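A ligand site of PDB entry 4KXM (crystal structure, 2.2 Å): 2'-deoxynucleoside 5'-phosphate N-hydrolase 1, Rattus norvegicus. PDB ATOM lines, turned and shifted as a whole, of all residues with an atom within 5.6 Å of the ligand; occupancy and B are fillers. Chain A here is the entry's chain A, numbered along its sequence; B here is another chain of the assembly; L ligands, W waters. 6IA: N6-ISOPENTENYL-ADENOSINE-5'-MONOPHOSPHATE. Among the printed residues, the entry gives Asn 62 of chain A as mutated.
OH of Tyr 6 touches O2' of the ligand, 3.8 Å away.
Cys 8 touches the ligand (CA to O3', 3.5 Å).
Ser 10 touches the ligand.
Val 39 touches the ligand (CG2 to O2', 3.6 Å).
Ile 58 touches the ligand.
Val 83 touches the ligand.
CB of Ala 111 of chain B touches N7 of the ligand, at 3.7 Å.
Met 112 of chain B touches the ligand (CG to O4', 3.2 Å).
Hydrophobic or aromatic side chains that line the ligand: Ile 11, His 38, Val 39, Ile 58, Ala 111 of chain B and Met 112 of chain B.
Of the 24 residues printed, 18 come within 4 Å of the ligand.
The side-chain hydroxyl (OG) of Ser 80 lies close to the backbone NH (N) of Gly 82, at 3.4 Å.
The side-chain hydroxyl of Ser 80 lies within hydrogen-bond range of the backbone NH of Val 83 (3.2 Å).
The side-chain hydroxyl (OG) of Ser 110 of chain B lies close to the backbone NH (N) of Met 112 of chain B (3.3 Å).
The side-chain sulfur (SG) of Cys 8 sits close to the side-chain carboxylate (OE2) of Glu 86.
OE1 of Glu 86 sits at hydrogen-bond distance from OH of Tyr 6, at 2.5 Å.
ND2 of Asn 62 lies within hydrogen-bond range of SD of Met 112 of chain B, at 3.3 Å.
OD1 of Asn 62 lies within hydrogen-bond range of NE2 of Gln 61 (3.2 Å).
The side-chain hydroxyl (OG) of Ser 10 is in hydrogen-bond range of the backbone carbonyl oxygen (O) of Gly 14 (2.7 Å).
Water W1 bridges OP2 of the ligand (2.6 Å) and N of Leu 81 (2.9 Å).
Water W2 lies within hydrogen-bond range of OP3 of the ligand (2.7 Å), N of Ala 111 of chain B (2.9 Å) and NE of Arg 12 (3.5 Å).
The side-chain hydroxyl of Ser 80 is in hydrogen-bond range of an oxygen (OP1) of the ligand, 2.5 Å away.
An oxygen (OP2) of the ligand sits at hydrogen-bond distance from the side-chain hydroxyl (OG) of Ser 110 of chain B (2.6 Å).
The backbone NH (N) of Arg 12 sits at hydrogen-bond distance from an oxygen (OP3) of the ligand (2.7 Å).
O2' of the ligand lies within hydrogen-bond range of OE1 of Glu 86, 2.7 Å away.
N of Ile 11 sits at hydrogen-bond distance from OP1 of the ligand.
The backbone NH (N) of Gly 82 lies within hydrogen-bond range of an oxygen (OP2) of the ligand.
N3 of the ligand is in hydrogen-bond range of NE2 of His 38, 3.0 Å away.
N of Gly 13 lies within hydrogen-bond range of OP1 of the ligand (3.0 Å).
The side-chain amide nitrogen (ND2) of Asn 62 is in hydrogen-bond range of a nitrogen (N3) of the ligand (3.1 Å).
The backbone NH (N) of Gly 9 is in hydrogen-bond range of an oxygen (O3') of the ligand (3.2 Å).
O of Gly 9 lies close to O3' of the ligand (3.2 Å).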
ATOM      1  N   TYR A   6     -20.724  12.845  -5.830  1.00  0.00           N
ATOM      2  CA  TYR A   6     -21.815  13.786  -6.005  1.00  0.00           C
ATOM      3  C   TYR A   6     -22.699  13.740  -4.750  1.00  0.00           C
ATOM      4  O   TYR A   6     -23.296  12.708  -4.449  1.00  0.00           O
ATOM      5  CB  TYR A   6     -22.631  13.402  -7.238  1.00  0.00           C
ATOM      6  CG  TYR A   6     -23.597  14.463  -7.730  1.00  0.00           C
ATOM      7  CD1 TYR A   6     -23.288  15.248  -8.833  1.00  0.00           C
ATOM      8  CD2 TYR A   6     -24.825  14.668  -7.099  1.00  0.00           C
ATOM      9  CE1 TYR A   6     -24.166  16.212  -9.307  1.00  0.00           C
ATOM     10  CE2 TYR A   6     -25.707  15.633  -7.559  1.00  0.00           C
ATOM     11  CZ  TYR A   6     -25.369  16.409  -8.661  1.00  0.00           C
ATOM     12  OH  TYR A   6     -26.241  17.361  -9.132  1.00  0.00           O
ATOM     13  N   PHE A   7     -22.768  14.855  -4.032  1.00  0.00           N
ATOM     14  CA  PHE A   7     -23.665  14.937  -2.869  1.00  0.00           C
ATOM     15  C   PHE A   7     -24.962  15.688  -3.187  1.00  0.00           C
ATOM     16  O   PHE A   7     -24.928  16.807  -3.705  1.00  0.00           O
ATOM     17  CB  PHE A   7     -22.970  15.548  -1.641  1.00  0.00           C
ATOM     18  CG  PHE A   7     -23.916  15.775  -0.479  1.00  0.00           C
ATOM     19  CD1 PHE A   7     -24.240  17.068  -0.080  1.00  0.00           C
ATOM     20  CD2 PHE A   7     -24.513  14.698   0.173  1.00  0.00           C
ATOM     21  CE1 PHE A   7     -25.134  17.281   0.966  1.00  0.00           C
ATOM     22  CE2 PHE A   7     -25.409  14.899   1.211  1.00  0.00           C
ATOM     23  CZ  PHE A   7     -25.716  16.196   1.623  1.00  0.00           C
ATOM     24  N   CYS A   8     -26.093  15.070  -2.873  1.00  0.00           N
ATOM     25  CA  CYS A   8     -27.423  15.683  -3.038  1.00  0.00           C
ATOM     26  C   CYS A   8     -27.992  16.116  -1.696  1.00  0.00           C
ATOM     27  O   CYS A   8     -27.931  15.368  -0.717  1.00  0.00           O
ATOM     28  CB  CYS A   8     -28.409  14.703  -3.683  1.00  0.00           C
ATOM     29  SG  CYS A   8     -27.780  13.825  -5.116  1.00  0.00           S
ATOM     30  N   GLY A   9     -28.567  17.312  -1.651  1.00  0.00           N
ATOM     31  CA  GLY A   9     -29.250  17.807  -0.459  1.00  0.00           C
ATOM     32  C   GLY A   9     -30.167  18.934  -0.836  1.00  0.00           C
ATOM     33  O   GLY A   9     -29.879  19.691  -1.759  1.00  0.00           O
ATOM     34  N   SER A  10     -31.294  19.055  -0.132  1.00  0.00           N
ATOM     35  CA  SER A  10     -32.305  20.065  -0.442  1.00  0.00           C
ATOM     36  C   SER A  10     -31.766  21.494  -0.427  1.00  0.00           C
ATOM     37  O   SER A  10     -31.003  21.882   0.471  1.00  0.00           O
ATOM     38  CB  SER A  10     -33.460  19.934   0.556  1.00  0.00           C
ATOM     39  OG  SER A  10     -34.378  21.002   0.435  1.00  0.00           O
ATOM     40  N   ILE A  11     -32.169  22.284  -1.426  1.00  0.00           N
ATOM     41  CA  ILE A  11     -31.879  23.727  -1.452  1.00  0.00           C
ATOM     42  C   ILE A  11     -33.185  24.532  -1.508  1.00  0.00           C
ATOM     43  O   ILE A  11     -33.595  25.097  -0.503  1.00  0.00           O
ATOM     44  CB  ILE A  11     -30.860  24.127  -2.573  1.00  0.00           C
ATOM     45  CG1 ILE A  11     -29.521  23.386  -2.340  1.00  0.00           C
ATOM     46  CG2 ILE A  11     -30.654  25.655  -2.601  1.00  0.00           C
ATOM     47  CD1 ILE A  11     -28.421  23.598  -3.396  1.00  0.00           C
ATOM     48  N   ARG A  12     -33.848  24.557  -2.657  1.00  0.00           N
ATOM     49  CA  ARG A  12     -35.136  25.243  -2.739  1.00  0.00           C
ATOM     50  C   ARG A  12     -36.305  24.431  -2.137  1.00  0.00           C
ATOM     51  O   ARG A  12     -37.397  24.943  -2.000  1.00  0.00           O
ATOM     52  CB  ARG A  12     -35.424  25.716  -4.166  1.00  0.00           C
ATOM     53  CG  ARG A  12     -34.570  26.921  -4.553  1.00  0.00           C
ATOM     54  CD  ARG A  12     -34.783  27.315  -5.997  1.00  0.00           C
ATOM     55  NE  ARG A  12     -33.788  28.289  -6.446  1.00  0.00           N
ATOM     56  CZ  ARG A  12     -33.551  28.591  -7.724  1.00  0.00           C
ATOM     57  NH1 ARG A  12     -34.236  28.001  -8.690  1.00  0.00           N
ATOM     58  NH2 ARG A  12     -32.616  29.481  -8.038  1.00  0.00           N
ATOM     59  N   GLY A  13     -36.038  23.178  -1.771  1.00  0.00           N
ATOM     60  CA  GLY A  13     -36.964  22.390  -0.977  1.00  0.00           C
ATOM     61  C   GLY A  13     -36.917  22.764   0.507  1.00  0.00           C
ATOM     62  O   GLY A  13     -37.745  22.313   1.305  1.00  0.00           O
ATOM     63  N   GLY A  14     -35.936  23.599   0.877  1.00  0.00           N
ATOM     64  CA  GLY A  14     -35.747  24.025   2.254  1.00  0.00           C
ATOM     65  C   GLY A  14     -34.339  23.748   2.758  1.00  0.00           C
ATOM     66  O   GLY A  14     -33.726  22.738   2.396  1.00  0.00           O
ATOM     67  N   THR A  36     -20.146  18.672  -5.540  1.00  0.00           N
ATOM     68  CA  THR A  36     -21.292  19.536  -5.268  1.00  0.00           C
ATOM     69  C   THR A  36     -21.175  20.231  -3.899  1.00  0.00           C
ATOM     70  O   THR A  36     -22.100  20.152  -3.069  1.00  0.00           O
ATOM     71  CB  THR A  36     -22.591  18.724  -5.316  1.00  0.00           C
ATOM     72  OG1 THR A  36     -22.457  17.595  -4.434  1.00  0.00           O
ATOM     73  CG2 THR A  36     -22.863  18.208  -6.721  1.00  0.00           C
ATOM     74  N   HIS A  38     -21.462  23.269  -3.213  1.00  0.00           N
ATOM     75  CA  HIS A  38     -22.471  24.335  -3.088  1.00  0.00           C
ATOM     76  C   HIS A  38     -23.647  23.959  -2.186  1.00  0.00           C
ATOM     77  O   HIS A  38     -24.229  24.832  -1.555  1.00  0.00           O
ATOM     78  CB  HIS A  38     -23.006  24.719  -4.468  1.00  0.00           C
ATOM     79  CG  HIS A  38     -23.389  23.541  -5.316  1.00  0.00           C
ATOM     80  ND1 HIS A  38     -22.691  23.168  -6.435  1.00  0.00           N
ATOM     81  CD2 HIS A  38     -24.402  22.644  -5.181  1.00  0.00           C
ATOM     82  CE1 HIS A  38     -23.262  22.104  -6.977  1.00  0.00           C
ATOM     83  NE2 HIS A  38     -24.294  21.762  -6.233  1.00  0.00           N
ATOM     84  N   VAL A  39     -23.986  22.667  -2.132  1.00  0.00           N
ATOM     85  CA  VAL A  39     -25.138  22.200  -1.337  1.00  0.00           C
ATOM     86  C   VAL A  39     -24.962  22.560   0.144  1.00  0.00           C
ATOM     87  O   VAL A  39     -25.939  22.833   0.849  1.00  0.00           O
ATOM     88  CB  VAL A  39     -25.403  20.675  -1.484  1.00  0.00           C
ATOM     89  CG1 VAL A  39     -26.668  20.283  -0.743  1.00  0.00           C
ATOM     90  CG2 VAL A  39     -25.530  20.264  -2.946  1.00  0.00           C
ATOM     91  N   ILE A  58     -27.170  25.910 -14.129  1.00  0.00           N
ATOM     92  CA  ILE A  58     -27.055  25.027 -12.970  1.00  0.00           C
ATOM     93  C   ILE A  58     -27.350  23.565 -13.316  1.00  0.00           C
ATOM     94  O   ILE A  58     -26.606  22.661 -12.916  1.00  0.00           O
ATOM     95  CB  ILE A  58     -27.945  25.515 -11.791  1.00  0.00           C
ATOM     96  CG1 ILE A  58     -27.416  26.851 -11.247  1.00  0.00           C
ATOM     97  CG2 ILE A  58     -28.016  24.442 -10.679  1.00  0.00           C
ATOM     98  CD1 ILE A  58     -28.490  27.720 -10.598  1.00  0.00           C
ATOM     99  N   GLN A  61     -24.440  22.202 -15.481  1.00  0.00           N
ATOM    100  CA  GLN A  61     -23.239  22.076 -14.642  1.00  0.00           C
ATOM    101  C   GLN A  61     -23.339  20.821 -13.766  1.00  0.00           C
ATOM    102  O   GLN A  61     -22.418  20.012 -13.733  1.00  0.00           O
ATOM    103  CB  GLN A  61     -23.096  23.322 -13.761  1.00  0.00           C
ATOM    104  CG  GLN A  61     -21.962  23.265 -12.739  1.00  0.00           C
ATOM    105  CD  GLN A  61     -22.139  24.290 -11.612  1.00  0.00           C
ATOM    106  OE1 GLN A  61     -21.366  25.235 -11.505  1.00  0.00           O
ATOM    107  NE2 GLN A  61     -23.158  24.088 -10.783  1.00  0.00           N
ATOM    108  N   ASN A  62     -24.475  20.669 -13.095  1.00  0.00           N
ATOM    109  CA  ASN A  62     -24.732  19.554 -12.209  1.00  0.00           C
ATOM    110  C   ASN A  62     -24.845  18.204 -12.934  1.00  0.00           C
ATOM    111  O   ASN A  62     -24.373  17.181 -12.420  1.00  0.00           O
ATOM    112  CB  ASN A  62     -25.971  19.818 -11.362  1.00  0.00           C
ATOM    113  CG  ASN A  62     -25.735  20.832 -10.240  1.00  0.00           C
ATOM    114  OD1 ASN A  62     -24.636  21.354 -10.061  1.00  0.00           O
ATOM    115  ND2 ASN A  62     -26.774  21.107  -9.488  1.00  0.00           N
ATOM    116  N   PRO A  79     -37.811  16.800   1.772  1.00  0.00           N
ATOM    117  CA  PRO A  79     -38.341  16.592   0.426  1.00  0.00           C
ATOM    118  C   PRO A  79     -37.864  17.676  -0.539  1.00  0.00           C
ATOM    119  O   PRO A  79     -37.903  18.866  -0.216  1.00  0.00           O
ATOM    120  CB  PRO A  79     -39.862  16.635   0.611  1.00  0.00           C
ATOM    121  CG  PRO A  79     -40.083  16.300   2.073  1.00  0.00           C
ATOM    122  CD  PRO A  79     -38.886  16.887   2.791  1.00  0.00           C
ATOM    123  N   SER A  80     -37.380  17.244  -1.707  1.00  0.00           N
ATOM    124  CA  SER A  80     -36.785  18.146  -2.669  1.00  0.00           C
ATOM    125  C   SER A  80     -36.938  17.565  -4.063  1.00  0.00           C
ATOM    126  O   SER A  80     -36.550  16.419  -4.317  1.00  0.00           O
ATOM    127  CB  SER A  80     -35.297  18.344  -2.344  1.00  0.00           C
ATOM    128  OG  SER A  80     -34.610  18.944  -3.424  1.00  0.00           O
ATOM    129  N   LEU A  81     -37.481  18.379  -4.951  1.00  0.00           N
ATOM    130  CA  LEU A  81     -37.585  18.058  -6.389  1.00  0.00           C
ATOM    131  C   LEU A  81     -36.219  17.756  -7.009  1.00  0.00           C
ATOM    132  O   LEU A  81     -36.074  16.789  -7.756  1.00  0.00           O
ATOM    133  CB  LEU A  81     -38.211  19.244  -7.123  1.00  0.00           C
ATOM    134  CG  LEU A  81     -39.686  19.386  -7.529  1.00  0.00           C
ATOM    135  CD1 LEU A  81     -40.667  18.343  -6.983  1.00  0.00           C
ATOM    136  CD2 LEU A  81     -40.173  20.805  -7.239  1.00  0.00           C
ATOM    137  N   GLY A  82     -35.235  18.613  -6.699  1.00  0.00           N
ATOM    138  CA  GLY A  82     -33.902  18.530  -7.281  1.00  0.00           C
ATOM    139  C   GLY A  82     -33.138  17.293  -6.850  1.00  0.00           C
ATOM    140  O   GLY A  82     -32.501  16.643  -7.677  1.00  0.00           O
ATOM    141  N   VAL A  83     -33.197  16.984  -5.554  1.00  0.00           N
ATOM    142  CA  VAL A  83     -32.597  15.785  -4.998  1.00  0.00           C
ATOM    143  C   VAL A  83     -33.230  14.546  -5.631  1.00  0.00           C
ATOM    144  O   VAL A  83     -32.514  13.639  -6.071  1.00  0.00           O
ATOM    145  CB  VAL A  83     -32.711  15.714  -3.450  1.00  0.00           C
ATOM    146  CG1 VAL A  83     -32.149  14.408  -2.916  1.00  0.00           C
ATOM    147  CG2 VAL A  83     -32.002  16.881  -2.805  1.00  0.00           C
ATOM    148  N   GLU A  86     -31.993  14.335  -9.246  1.00  0.00           N
ATOM    149  CA  GLU A  86     -30.614  13.858  -9.289  1.00  0.00           C
ATOM    150  C   GLU A  86     -30.529  12.349  -9.054  1.00  0.00           C
ATOM    151  O   GLU A  86     -29.745  11.663  -9.692  1.00  0.00           O
ATOM    152  CB  GLU A  86     -29.740  14.614  -8.281  1.00  0.00           C
ATOM    153  CG  GLU A  86     -29.418  16.028  -8.703  1.00  0.00           C
ATOM    154  CD  GLU A  86     -29.047  16.941  -7.548  1.00  0.00           C
ATOM    155  OE1 GLU A  86     -28.303  17.911  -7.778  1.00  0.00           O
ATOM    156  OE2 GLU A  86     -29.496  16.694  -6.399  1.00  0.00           O
ATOM    157  N   SER B 110     -37.327  24.619  -8.003  1.00  0.00           N
ATOM    158  CA  SER B 110     -36.038  23.946  -8.122  1.00  0.00           C
ATOM    159  C   SER B 110     -35.290  24.279  -9.414  1.00  0.00           C
ATOM    160  O   SER B 110     -35.821  24.076 -10.509  1.00  0.00           O
ATOM    161  CB  SER B 110     -36.229  22.430  -8.039  1.00  0.00           C
ATOM    162  OG  SER B 110     -35.015  21.745  -8.292  1.00  0.00           O
ATOM    163  N   ALA B 111     -34.069  24.793  -9.270  1.00  0.00           N
ATOM    164  CA  ALA B 111     -33.166  25.031 -10.404  1.00  0.00           C
ATOM    165  C   ALA B 111     -32.984  23.789 -11.303  1.00  0.00           C
ATOM    166  O   ALA B 111     -32.885  23.910 -12.517  1.00  0.00           O
ATOM    167  CB  ALA B 111     -31.813  25.525  -9.922  1.00  0.00           C
ATOM    168  N   MET B 112     -32.959  22.603 -10.681  1.00  0.00           N
ATOM    169  CA  MET B 112     -32.786  21.366 -11.427  1.00  0.00           C
ATOM    170  C   MET B 112     -34.030  21.032 -12.255  1.00  0.00           C
ATOM    171  O   MET B 112     -33.914  20.342 -13.271  1.00  0.00           O
ATOM    172  CB  MET B 112     -32.428  20.201 -10.504  1.00  0.00           C
ATOM    173  CG  MET B 112     -31.065  20.345  -9.829  1.00  0.00           C
ATOM    174  SD  MET B 112     -29.665  20.440 -10.986  1.00  0.00           S
ATOM    175  CE  MET B 112     -29.651  18.752 -11.623  1.00  0.00           C
HETATM  176  OP3 6IA L   1     -33.248  23.213  -4.925  1.00  0.00           O
HETATM  177  P   6IA L   1     -33.737  21.691  -4.704  1.00  0.00           P
HETATM  178  OP1 6IA L   1     -34.130  21.397  -3.313  1.00  0.00           O
HETATM  179  OP2 6IA L   1     -34.910  21.438  -5.744  1.00  0.00           O
HETATM  180  O5' 6IA L   1     -32.553  20.731  -5.211  1.00  0.00           O
HETATM  181  C5' 6IA L   1     -31.291  20.751  -4.598  1.00  0.00           C
HETATM  182  C4' 6IA L   1     -30.333  19.926  -5.434  1.00  0.00           C
HETATM  183  O4' 6IA L   1     -30.187  20.457  -6.782  1.00  0.00           O
HETATM  184  C3' 6IA L   1     -28.979  19.948  -4.770  1.00  0.00           C
HETATM  185  O3' 6IA L   1     -28.637  18.591  -4.538  1.00  0.00           O
HETATM  186  C2' 6IA L   1     -28.017  20.606  -5.761  1.00  0.00           C
HETATM  187  O2' 6IA L   1     -27.007  19.679  -6.183  1.00  0.00           O
HETATM  188  C1' 6IA L   1     -28.879  21.036  -6.964  1.00  0.00           C
HETATM  189  N9  6IA L   1     -29.013  22.508  -6.983  1.00  0.00           N
HETATM  190  C8  6IA L   1     -30.155  23.200  -6.834  1.00  0.00           C
HETATM  191  N7  6IA L   1     -29.871  24.504  -6.884  1.00  0.00           N
HETATM  192  C5  6IA L   1     -28.556  24.658  -7.048  1.00  0.00           C
HETATM  193  C6  6IA L   1     -27.713  25.754  -7.165  1.00  0.00           C
HETATM  194  N6  6IA L   1     -28.179  27.009  -7.119  1.00  0.00           N
HETATM  195  N1  6IA L   1     -26.400  25.531  -7.338  1.00  0.00           N
HETATM  196  C2  6IA L   1     -25.911  24.303  -7.393  1.00  0.00           C
HETATM  197  N3  6IA L   1     -26.686  23.240  -7.287  1.00  0.00           N
HETATM  198  C4  6IA L   1     -28.011  23.383  -7.120  1.00  0.00           C
HETATM  199  C12 6IA L   1     -27.373  28.135  -6.567  1.00  0.00           C
HETATM  200  C13 6IA L   1     -26.547  28.674  -7.548  1.00  0.00           C
HETATM  201  C14 6IA L   1     -25.153  28.553  -7.710  1.00  0.00           C
HETATM  202  C15 6IA L   1     -24.289  27.735  -6.722  1.00  0.00           C
HETATM  203  C16 6IA L   1     -24.453  29.253  -8.880  1.00  0.00           C
HETATM  204  O   HOH W   1     -37.276  21.291  -4.610  1.00  0.00           O
HETATM  205  O   HOH W   2     -32.657  25.038  -6.799  1.00  0.00           O
